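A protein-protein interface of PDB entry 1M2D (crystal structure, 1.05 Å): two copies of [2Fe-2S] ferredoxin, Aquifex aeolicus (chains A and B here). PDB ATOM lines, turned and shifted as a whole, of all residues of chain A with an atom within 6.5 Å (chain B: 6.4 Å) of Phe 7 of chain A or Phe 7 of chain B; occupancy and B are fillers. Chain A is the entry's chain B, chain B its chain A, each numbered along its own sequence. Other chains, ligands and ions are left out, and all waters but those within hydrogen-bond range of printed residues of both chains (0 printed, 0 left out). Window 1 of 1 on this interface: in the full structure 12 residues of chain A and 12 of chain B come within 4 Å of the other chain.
OH of Tyr 68 of chain B sits at hydrogen-bond distance from ND1 of His 5 of chain A (3.0 Å).
ND1 of His 5 of chain B is in hydrogen-bond range of OH of Tyr 68 of chain A (3.0 Å).
His 5 of chain A touches Met 56 of chain B, and with the chains exchanged Met 56 of chain A touches His 5 of chain B.
Phe 7 of chain B touches its own counterpart, Phe 7 of chain A.
Thr 51 of chain A touches Thr 53 of chain B, and with the chains exchanged Thr 53 of chain A touches Thr 51 of chain B.
Pro 52 of chain A touches Thr 53 of chain B, and with the chains exchanged Thr 53 of chain A touches Pro 52 of chain B.
16 positions are printed for both chains.
Of the 14 pairs that touch across the chains among the printed residues, 14 have their exchanged pair printed and touching as well.
N of Thr 53 of chain A sits at hydrogen-bond distance from O of Val 8 of chain A, at 2.9 Å.
The backbone NH of Val 8 of chain A is in hydrogen-bond range of the backbone carbonyl oxygen of Thr 51 of chain A (2.9 Å).
The backbone carbonyl oxygen (O) of Val 8 of chain B lies within hydrogen-bond range of the backbone NH (N) of Thr 53 of chain B.
The backbone NH (N) of Val 8 of chain B sits at hydrogen-bond distance from the backbone carbonyl oxygen (O) of Thr 51 of chain B.
OG1 of Thr 51 of chain A is in hydrogen-bond range of NE2 of His 5 of chain A (2.8 Å).
The backbone NH (N) of Phe 7 of chain B lies within hydrogen-bond range of the backbone carbonyl oxygen (O) of Val 66 of chain B (2.8 Å).
Among the printed residues, merely in contact across the chains: His 5 of chain A with Met 56 of chain B (3.9 Å), Phe 7 of chain A with Phe 7 of chain B (3.4 Å), Phe 7 of chain A with Tyr 68 of chain B (3.7 Å), Thr 51 of chain A with Thr 53 of chain B (3.6 Å), Thr 51 of chain A with Met 56 of chain B (3.7 Å), Pro 52 of chain A with Thr 53 of chain B (3.4 Å), Thr 53 of chain A with Thr 51 of chain B (3.7 Å), Thr 53 of chain A with Pro 52 of chain B (3.5 Å), Met 56 of chain A with His 5 of chain B (3.9 Å), Met 56 of chain A with Thr 51 of chain B (3.7 Å), Tyr 68 of chain A with Phe 7 of chain B (3.7 Å) and Tyr 68 of chain A with Tyr 68 of chain B (3.5 Å).
Hydrophobic or aromatic side chains of chain B within 4 Å of the printed part of chain A: His 5, Phe 7, Met 56 and Tyr 68.
Of the 16 printed residues of chain A, 7 touch a printed residue of chain B.
Printed residues of chain A that touch a printed residue of chain B: His 5, Phe 7, Thr 51, Pro 52, Thr 53, Met 56 and Tyr 68.
Hydrophobic or aromatic side chains of chain A within 4 Å of the printed part of chain B: His 5, Phe 7, Met 56 and Tyr 68.
Along chain A the printed residues that touch a printed residue of chain B span positions 5 to 68.
Among the printed residues, no Asp or Glu carboxylate lies within 4 Å of a Lys or Arg side-chain nitrogen of the other chain.
Of the printed residues of chain B, His 5 of chain A touches Met 56 and Tyr 68.
Phe 7 of chain A touches two residues of chain B.
Cys 9 of chain A touches none of the printed residues of chain B.
Printed residues of chain B within 4 Å of Thr 51 of chain A: Thr 53 and Met 56.
Of the printed residues of chain B, Pro 52 of chain A touches Thr 53 (3.4 Å).
Of the printed residues of chain B, Met 56 of chain A touches His 5 (3.9 Å) and Thr 51 (3.7 Å).
Of the printed residues of chain A, Phe 7 of chain B touches Phe 7 (3.4 Å) and Tyr 68 (3.7 Å).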
ATOM      1  N   HIS A   5     -10.854  26.254  13.079  1.00  0.00           N
ATOM      2  CA  HIS A   5     -12.173  26.169  13.671  1.00  0.00           C
ATOM      3  C   HIS A   5     -12.291  27.337  14.654  1.00  0.00           C
ATOM      4  O   HIS A   5     -11.559  27.396  15.637  1.00  0.00           O
ATOM      5  CB  HIS A   5     -12.349  24.818  14.377  1.00  0.00           C
ATOM      6  CG  HIS A   5     -13.807  24.475  14.594  1.00  0.00           C
ATOM      7  ND1 HIS A   5     -14.306  23.255  14.752  1.00  0.00           N
ATOM      8  CD2 HIS A   5     -14.906  25.246  14.642  1.00  0.00           C
ATOM      9  CE1 HIS A   5     -15.503  23.125  14.993  1.00  0.00           C
ATOM     10  NE2 HIS A   5     -15.964  24.387  14.886  1.00  0.00           N
ATOM     11  N   VAL A   6     -13.176  28.261  14.350  1.00  0.00           N
ATOM     12  CA  VAL A   6     -13.387  29.484  15.118  1.00  0.00           C
ATOM     13  C   VAL A   6     -14.659  29.341  15.918  1.00  0.00           C
ATOM     14  O   VAL A   6     -15.715  29.073  15.327  1.00  0.00           O
ATOM     15  CB  VAL A   6     -13.466  30.705  14.207  1.00  0.00           C
ATOM     16  CG1 VAL A   6     -13.646  31.965  15.008  1.00  0.00           C
ATOM     17  CG2 VAL A   6     -12.249  30.811  13.284  1.00  0.00           C
ATOM     18  N   PHE A   7     -14.579  29.553  17.217  1.00  0.00           N
ATOM     19  CA  PHE A   7     -15.691  29.491  18.141  1.00  0.00           C
ATOM     20  C   PHE A   7     -15.969  30.894  18.670  1.00  0.00           C
ATOM     21  O   PHE A   7     -15.072  31.532  19.201  1.00  0.00           O
ATOM     22  CB  PHE A   7     -15.393  28.560  19.298  1.00  0.00           C
ATOM     23  CG  PHE A   7     -15.291  27.117  18.829  1.00  0.00           C
ATOM     24  CD1 PHE A   7     -14.083  26.566  18.469  1.00  0.00           C
ATOM     25  CD2 PHE A   7     -16.413  26.328  18.768  1.00  0.00           C
ATOM     26  CE1 PHE A   7     -13.972  25.239  18.081  1.00  0.00           C
ATOM     27  CE2 PHE A   7     -16.331  24.984  18.385  1.00  0.00           C
ATOM     28  CZ  PHE A   7     -15.095  24.436  18.070  1.00  0.00           C
ATOM     29  N   VAL A   8     -17.195  31.356  18.492  1.00  0.00           N
ATOM     30  CA  VAL A   8     -17.606  32.684  18.930  1.00  0.00           C
ATOM     31  C   VAL A   8     -18.683  32.498  20.009  1.00  0.00           C
ATOM     32  O   VAL A   8     -19.742  31.953  19.716  1.00  0.00           O
ATOM     33  CB  VAL A   8     -18.134  33.549  17.795  1.00  0.00           C
ATOM     34  CG1 VAL A   8     -18.511  34.925  18.312  1.00  0.00           C
ATOM     35  CG2 VAL A   8     -17.133  33.604  16.655  1.00  0.00           C
ATOM     36  N   CYS A   9     -18.427  32.997  21.221  1.00  0.00           N
ATOM     37  CA  CYS A   9     -19.453  32.959  22.230  1.00  0.00           C
ATOM     38  C   CYS A   9     -20.574  33.929  21.858  1.00  0.00           C
ATOM     39  O   CYS A   9     -20.337  35.102  21.689  1.00  0.00           O
ATOM     40  CB  CYS A   9     -18.860  33.331  23.603  1.00  0.00           C
ATOM     41  SG  CYS A   9     -20.139  33.324  24.877  1.00  0.00           S
ATOM     42  N   VAL A  49     -14.315  26.628   9.741  1.00  0.00           N
ATOM     43  CA  VAL A  49     -15.632  26.458  10.323  1.00  0.00           C
ATOM     44  C   VAL A  49     -15.818  27.574  11.356  1.00  0.00           C
ATOM     45  O   VAL A  49     -14.886  27.802  12.112  1.00  0.00           O
ATOM     46  CB  VAL A  49     -15.826  25.082  10.973  1.00  0.00           C
ATOM     47  CG1 VAL A  49     -17.185  24.949  11.629  1.00  0.00           C
ATOM     48  CG2 VAL A  49     -15.633  23.979   9.922  1.00  0.00           C
ATOM     49  N   ILE A  50     -17.000  28.176  11.399  1.00  0.00           N
ATOM     50  CA  ILE A  50     -17.361  29.191  12.384  1.00  0.00           C
ATOM     51  C   ILE A  50     -18.533  28.634  13.157  1.00  0.00           C
ATOM     52  O   ILE A  50     -19.562  28.298  12.599  1.00  0.00           O
ATOM     53  CB  ILE A  50     -17.745  30.513  11.736  1.00  0.00           C
ATOM     54  CG1 ILE A  50     -16.791  31.037  10.673  1.00  0.00           C
ATOM     55  CG2 ILE A  50     -18.014  31.578  12.781  1.00  0.00           C
ATOM     56  CD1 ILE A  50     -15.364  31.303  11.193  1.00  0.00           C
ATOM     57  N   THR A  51     -18.359  28.515  14.486  1.00  0.00           N
ATOM     58  CA  THR A  51     -19.345  27.870  15.330  1.00  0.00           C
ATOM     59  C   THR A  51     -19.741  28.806  16.487  1.00  0.00           C
ATOM     60  O   THR A  51     -18.854  29.316  17.189  1.00  0.00           O
ATOM     61  CB  THR A  51     -18.823  26.576  15.925  1.00  0.00           C
ATOM     62  OG1 THR A  51     -18.390  25.688  14.861  1.00  0.00           O
ATOM     63  CG2 THR A  51     -19.789  25.862  16.820  1.00  0.00           C
ATOM     64  N   PRO A  52     -21.045  29.021  16.682  1.00  0.00           N
ATOM     65  CA  PRO A  52     -21.502  29.821  17.832  1.00  0.00           C
ATOM     66  C   PRO A  52     -21.568  28.951  19.078  1.00  0.00           C
ATOM     67  O   PRO A  52     -21.943  27.767  18.977  1.00  0.00           O
ATOM     68  CB  PRO A  52     -22.876  30.265  17.394  1.00  0.00           C
ATOM     69  CG  PRO A  52     -23.396  29.112  16.557  1.00  0.00           C
ATOM     70  CD  PRO A  52     -22.178  28.521  15.894  1.00  0.00           C
ATOM     71  N   THR A  53     -21.253  29.529  20.246  1.00  0.00           N
ATOM     72  CA  THR A  53     -21.233  28.771  21.459  1.00  0.00           C
ATOM     73  C   THR A  53     -21.951  29.475  22.594  1.00  0.00           C
ATOM     74  O   THR A  53     -22.215  30.675  22.568  1.00  0.00           O
ATOM     75  CB  THR A  53     -19.789  28.474  21.933  1.00  0.00           C
ATOM     76  OG1 THR A  53     -19.205  29.665  22.516  1.00  0.00           O
ATOM     77  CG2 THR A  53     -18.892  28.025  20.836  1.00  0.00           C
ATOM     78  N   MET A  56     -17.949  30.498  27.446  1.00  0.00           N
ATOM     79  CA  MET A  56     -16.628  29.865  27.553  1.00  0.00           C
ATOM     80  C   MET A  56     -15.844  30.387  28.761  1.00  0.00           C
ATOM     81  O   MET A  56     -14.608  30.194  28.846  1.00  0.00           O
ATOM     82  CB  MET A  56     -15.846  29.977  26.265  1.00  0.00           C
ATOM     83  CG  MET A  56     -16.476  29.139  25.176  1.00  0.00           C
ATOM     84  SD  MET A  56     -15.516  29.033  23.623  1.00  0.00           S
ATOM     85  CE  MET A  56     -15.903  30.592  22.849  1.00  0.00           C
ATOM     86  N   VAL A  64     -15.619  36.886  23.410  1.00  0.00           N
ATOM     87  CA  VAL A  64     -14.628  35.860  23.422  1.00  0.00           C
ATOM     88  C   VAL A  64     -14.715  35.033  22.119  1.00  0.00           C
ATOM     89  O   VAL A  64     -15.773  34.561  21.738  1.00  0.00           O
ATOM     90  CB  VAL A  64     -14.751  34.928  24.655  1.00  0.00           C
ATOM     91  CG1 VAL A  64     -13.736  33.793  24.627  1.00  0.00           C
ATOM     92  CG2 VAL A  64     -14.662  35.747  25.947  1.00  0.00           C
ATOM     93  N   VAL A  65     -13.559  34.875  21.498  1.00  0.00           N
ATOM     94  CA  VAL A  65     -13.411  34.120  20.270  1.00  0.00           C
ATOM     95  C   VAL A  65     -12.224  33.184  20.439  1.00  0.00           C
ATOM     96  O   VAL A  65     -11.166  33.663  20.835  1.00  0.00           O
ATOM     97  CB  VAL A  65     -13.178  35.053  19.054  1.00  0.00           C
ATOM     98  CG1 VAL A  65     -12.962  34.255  17.777  1.00  0.00           C
ATOM     99  CG2 VAL A  65     -14.374  35.999  18.892  1.00  0.00           C
ATOM    100  N   VAL A  66     -12.376  31.898  20.141  1.00  0.00           N
ATOM    101  CA  VAL A  66     -11.286  30.954  20.294  1.00  0.00           C
ATOM    102  C   VAL A  66     -11.017  30.282  18.952  1.00  0.00           C
ATOM    103  O   VAL A  66     -11.955  29.854  18.268  1.00  0.00           O
ATOM    104  CB  VAL A  66     -11.582  29.924  21.390  1.00  0.00           C
ATOM    105  CG1 VAL A  66     -10.363  29.038  21.632  1.00  0.00           C
ATOM    106  CG2 VAL A  66     -12.056  30.608  22.650  1.00  0.00           C
ATOM    107  N   VAL A  67      -9.754  30.201  18.556  1.00  0.00           N
ATOM    108  CA  VAL A  67      -9.346  29.585  17.321  1.00  0.00           C
ATOM    109  C   VAL A  67      -8.585  28.291  17.588  1.00  0.00           C
ATOM    110  O   VAL A  67      -7.555  28.327  18.276  1.00  0.00           O
ATOM    111  CB  VAL A  67      -8.493  30.526  16.480  1.00  0.00           C
ATOM    112  CG1 VAL A  67      -8.106  29.862  15.159  1.00  0.00           C
ATOM    113  CG2 VAL A  67      -9.178  31.874  16.221  1.00  0.00           C
ATOM    114  N   TYR A  68      -9.094  27.203  17.074  1.00  0.00           N
ATOM    115  CA  TYR A  68      -8.456  25.869  17.185  1.00  0.00           C
ATOM    116  C   TYR A  68      -8.064  25.406  15.801  1.00  0.00           C
ATOM    117  O   TYR A  68      -8.607  25.837  14.780  1.00  0.00           O
ATOM    118  CB  TYR A  68      -9.413  24.902  17.881  1.00  0.00           C
ATOM    119  CG  TYR A  68      -9.471  25.071  19.369  1.00  0.00           C
ATOM    120  CD1 TYR A  68     -10.633  25.452  20.024  1.00  0.00           C
ATOM    121  CD2 TYR A  68      -8.325  24.885  20.157  1.00  0.00           C
ATOM    122  CE1 TYR A  68     -10.692  25.616  21.406  1.00  0.00           C
ATOM    123  CE2 TYR A  68      -8.365  25.031  21.523  1.00  0.00           C
ATOM    124  CZ  TYR A  68      -9.559  25.391  22.118  1.00  0.00           C
ATOM    125  OH  TYR A  68      -9.411  25.527  23.436  1.00  0.00           O
ATOM    126  N   HIS B   5     -10.484  20.935  25.546  1.00  0.00           N
ATOM    127  CA  HIS B   5     -11.713  21.734  25.369  1.00  0.00           C
ATOM    128  C   HIS B   5     -12.667  20.847  24.577  1.00  0.00           C
ATOM    129  O   HIS B   5     -12.387  20.445  23.437  1.00  0.00           O
ATOM    130  CB  HIS B   5     -11.366  23.002  24.606  1.00  0.00           C
ATOM    131  CG  HIS B   5     -12.374  24.084  24.789  1.00  0.00           C
ATOM    132  ND1 HIS B   5     -12.194  25.386  24.641  1.00  0.00           N
ATOM    133  CD2 HIS B   5     -13.671  24.025  25.200  1.00  0.00           C
ATOM    134  CE1 HIS B   5     -13.139  26.125  24.790  1.00  0.00           C
ATOM    135  NE2 HIS B   5     -14.115  25.335  25.192  1.00  0.00           N
ATOM    136  N   VAL B   6     -13.780  20.504  25.217  1.00  0.00           N
ATOM    137  CA  VAL B   6     -14.774  19.612  24.662  1.00  0.00           C
ATOM    138  C   VAL B   6     -15.975  20.456  24.222  1.00  0.00           C
ATOM    139  O   VAL B   6     -16.520  21.216  25.052  1.00  0.00           O
ATOM    140  CB  VAL B   6     -15.248  18.575  25.703  1.00  0.00           C
ATOM    141  CG1 VAL B   6     -16.277  17.648  25.109  1.00  0.00           C
ATOM    142  CG2 VAL B   6     -14.048  17.815  26.253  1.00  0.00           C
ATOM    143  N   PHE B   7     -16.356  20.365  22.978  1.00  0.00           N
ATOM    144  CA  PHE B   7     -17.482  21.074  22.402  1.00  0.00           C
ATOM    145  C   PHE B   7     -18.588  20.072  22.098  1.00  0.00           C
ATOM    146  O   PHE B   7     -18.361  19.102  21.348  1.00  0.00           O
ATOM    147  CB  PHE B   7     -17.044  21.784  21.117  1.00  0.00           C
ATOM    148  CG  PHE B   7     -16.111  22.923  21.377  1.00  0.00           C
ATOM    149  CD1 PHE B   7     -14.727  22.742  21.315  1.00  0.00           C
ATOM    150  CD2 PHE B   7     -16.583  24.185  21.747  1.00  0.00           C
ATOM    151  CE1 PHE B   7     -13.860  23.779  21.585  1.00  0.00           C
ATOM    152  CE2 PHE B   7     -15.718  25.240  21.958  1.00  0.00           C
ATOM    153  CZ  PHE B   7     -14.347  25.046  21.868  1.00  0.00           C
ATOM    154  N   VAL B   8     -19.760  20.298  22.645  1.00  0.00           N
ATOM    155  CA  VAL B   8     -20.913  19.422  22.440  1.00  0.00           C
ATOM    156  C   VAL B   8     -21.995  20.222  21.704  1.00  0.00           C
ATOM    157  O   VAL B   8     -22.472  21.223  22.211  1.00  0.00           O
ATOM    158  CB  VAL B   8     -21.487  18.908  23.771  1.00  0.00           C
ATOM    159  CG1 VAL B   8     -22.640  17.965  23.507  1.00  0.00           C
ATOM    160  CG2 VAL B   8     -20.408  18.198  24.547  1.00  0.00           C
ATOM    161  N   CYS B   9     -22.365  19.753  20.503  1.00  0.00           N
ATOM    162  CA  CYS B   9     -23.452  20.401  19.783  1.00  0.00           C
ATOM    163  C   CYS B   9     -24.763  20.147  20.541  1.00  0.00           C
ATOM    164  O   CYS B   9     -25.121  18.994  20.750  1.00  0.00           O
ATOM    165  CB  CYS B   9     -23.539  19.883  18.376  1.00  0.00           C
ATOM    166  SG  CYS B   9     -24.931  20.644  17.487  1.00  0.00           S
ATOM    167  N   VAL B  49     -12.577  21.935  29.864  1.00  0.00           N
ATOM    168  CA  VAL B  49     -13.716  22.850  29.704  1.00  0.00           C
ATOM    169  C   VAL B  49     -14.709  22.159  28.783  1.00  0.00           C
ATOM    170  O   VAL B  49     -14.280  21.589  27.787  1.00  0.00           O
ATOM    171  CB  VAL B  49     -13.331  24.198  29.136  1.00  0.00           C
ATOM    172  CG1 VAL B  49     -14.547  25.010  28.758  1.00  0.00           C
ATOM    173  CG2 VAL B  49     -12.559  24.978  30.204  1.00  0.00           C
ATOM    174  N   ILE B  50     -15.986  22.226  29.080  1.00  0.00           N
ATOM    175  CA  ILE B  50     -17.080  21.671  28.336  1.00  0.00           C
ATOM    176  C   ILE B  50     -17.933  22.843  27.865  1.00  0.00           C
ATOM    177  O   ILE B  50     -18.442  23.604  28.674  1.00  0.00           O
ATOM    178  CB  ILE B  50     -18.002  20.683  29.118  1.00  0.00           C
ATOM    179  CG1 ILE B  50     -17.271  19.682  29.978  1.00  0.00           C
ATOM    180  CG2 ILE B  50     -18.912  19.982  28.120  1.00  0.00           C
ATOM    181  CD1 ILE B  50     -16.330  18.795  29.173  1.00  0.00           C
ATOM    182  N   THR B  51     -18.104  22.986  26.562  1.00  0.00           N
ATOM    183  CA  THR B  51     -18.800  24.115  25.955  1.00  0.00           C
ATOM    184  C   THR B  51     -19.911  23.622  25.064  1.00  0.00           C
ATOM    185  O   THR B  51     -19.675  22.812  24.176  1.00  0.00           O
ATOM    186  CB  THR B  51     -17.831  24.992  25.129  1.00  0.00           C
ATOM    187  OG1 THR B  51     -16.760  25.423  25.977  1.00  0.00           O
ATOM    188  CG2 THR B  51     -18.521  26.173  24.511  1.00  0.00           C
ATOM    189  N   PRO B  52     -21.151  24.135  25.241  1.00  0.00           N
ATOM    190  CA  PRO B  52     -22.234  23.803  24.325  1.00  0.00           C
ATOM    191  C   PRO B  52     -22.194  24.674  23.077  1.00  0.00           C
ATOM    192  O   PRO B  52     -21.857  25.847  23.184  1.00  0.00           O
ATOM    193  CB  PRO B  52     -23.499  24.117  25.181  1.00  0.00           C
ATOM    194  CG  PRO B  52     -23.054  25.269  26.044  1.00  0.00           C
ATOM    195  CD  PRO B  52     -21.578  25.076  26.304  1.00  0.00           C
ATOM    196  N   THR B  53     -22.569  24.101  21.939  1.00  0.00           N
ATOM    197  CA  THR B  53     -22.490  24.824  20.687  1.00  0.00           C
ATOM    198  C   THR B  53     -23.731  24.682  19.849  1.00  0.00           C
ATOM    199  O   THR B  53     -24.578  23.800  20.044  1.00  0.00           O
ATOM    200  CB  THR B  53     -21.300  24.364  19.783  1.00  0.00           C
ATOM    201  OG1 THR B  53     -21.600  23.117  19.178  1.00  0.00           O
ATOM    202  CG2 THR B  53     -20.038  24.177  20.607  1.00  0.00           C
ATOM    203  N   MET B  56     -22.423  22.071  14.130  1.00  0.00           N
ATOM    204  CA  MET B  56     -21.073  21.958  13.594  1.00  0.00           C
ATOM    205  C   MET B  56     -21.028  21.206  12.271  1.00  0.00           C
ATOM    206  O   MET B  56     -20.009  20.720  11.833  1.00  0.00           O
ATOM    207  CB  MET B  56     -20.116  21.336  14.634  1.00  0.00           C
ATOM    208  CG  MET B  56     -19.872  22.348  15.753  1.00  0.00           C
ATOM    209  SD  MET B  56     -18.618  21.819  16.966  1.00  0.00           S
ATOM    210  CE  MET B  56     -19.547  20.646  17.928  1.00  0.00           C
ATOM    211  N   VAL B  64     -22.721  15.167  17.861  1.00  0.00           N
ATOM    212  CA  VAL B  64     -21.351  15.564  17.506  1.00  0.00           C
ATOM    213  C   VAL B  64     -20.661  16.176  18.722  1.00  0.00           C
ATOM    214  O   VAL B  64     -21.186  17.124  19.338  1.00  0.00           O
ATOM    215  CB  VAL B  64     -21.354  16.531  16.319  1.00  0.00           C
ATOM    216  CG1 VAL B  64     -19.934  16.944  15.987  1.00  0.00           C
ATOM    217  CG2 VAL B  64     -22.015  15.884  15.096  1.00  0.00           C
ATOM    218  N   VAL B  65     -19.479  15.653  19.044  1.00  0.00           N
ATOM    219  CA  VAL B  65     -18.644  16.131  20.132  1.00  0.00           C
ATOM    220  C   VAL B  65     -17.240  16.308  19.578  1.00  0.00           C
ATOM    221  O   VAL B  65     -16.730  15.365  18.975  1.00  0.00           O
ATOM    222  CB  VAL B  65     -18.655  15.146  21.325  1.00  0.00           C
ATOM    223  CG1 VAL B  65     -17.699  15.637  22.387  1.00  0.00           C
ATOM    224  CG2 VAL B  65     -20.075  14.979  21.811  1.00  0.00           C
ATOM    225  N   VAL B  66     -16.619  17.464  19.782  1.00  0.00           N
ATOM    226  CA  VAL B  66     -15.280  17.721  19.248  1.00  0.00           C
ATOM    227  C   VAL B  66     -14.347  18.057  20.393  1.00  0.00           C
ATOM    228  O   VAL B  66     -14.692  18.861  21.258  1.00  0.00           O
ATOM    229  CB  VAL B  66     -15.334  18.856  18.205  1.00  0.00           C
ATOM    230  CG1 VAL B  66     -13.935  19.035  17.598  1.00  0.00           C
ATOM    231  CG2 VAL B  66     -16.408  18.559  17.178  1.00  0.00           C
ATOM    232  N   VAL B  67     -13.171  17.464  20.388  1.00  0.00           N
ATOM    233  CA  VAL B  67     -12.177  17.676  21.405  1.00  0.00           C
ATOM    234  C   VAL B  67     -10.968  18.382  20.806  1.00  0.00           C
ATOM    235  O   VAL B  67     -10.332  17.835  19.883  1.00  0.00           O
ATOM    236  CB  VAL B  67     -11.734  16.367  22.106  1.00  0.00           C
ATOM    237  CG1 VAL B  67     -10.753  16.643  23.213  1.00  0.00           C
ATOM    238  CG2 VAL B  67     -12.968  15.625  22.614  1.00  0.00           C
ATOM    239  N   TYR B  68     -10.673  19.560  21.330  1.00  0.00           N
ATOM    240  CA  TYR B  68      -9.502  20.339  20.957  1.00  0.00           C
ATOM    241  C   TYR B  68      -8.537  20.430  22.098  1.00  0.00           C
ATOM    242  O   TYR B  68      -8.942  20.277  23.259  1.00  0.00           O
ATOM    243  CB  TYR B  68      -9.933  21.732  20.427  1.00  0.00           C
ATOM    244  CG  TYR B  68     -10.492  21.692  19.016  1.00  0.00           C
ATOM    245  CD1 TYR B  68     -11.787  22.057  18.748  1.00  0.00           C
ATOM    246  CD2 TYR B  68      -9.708  21.289  17.948  1.00  0.00           C
ATOM    247  CE1 TYR B  68     -12.304  22.033  17.463  1.00  0.00           C
ATOM    248  CE2 TYR B  68     -10.206  21.250  16.670  1.00  0.00           C
ATOM    249  CZ  TYR B  68     -11.497  21.618  16.445  1.00  0.00           C
ATOM    250  OH  TYR B  68     -11.880  21.504  15.184  1.00  0.00           O
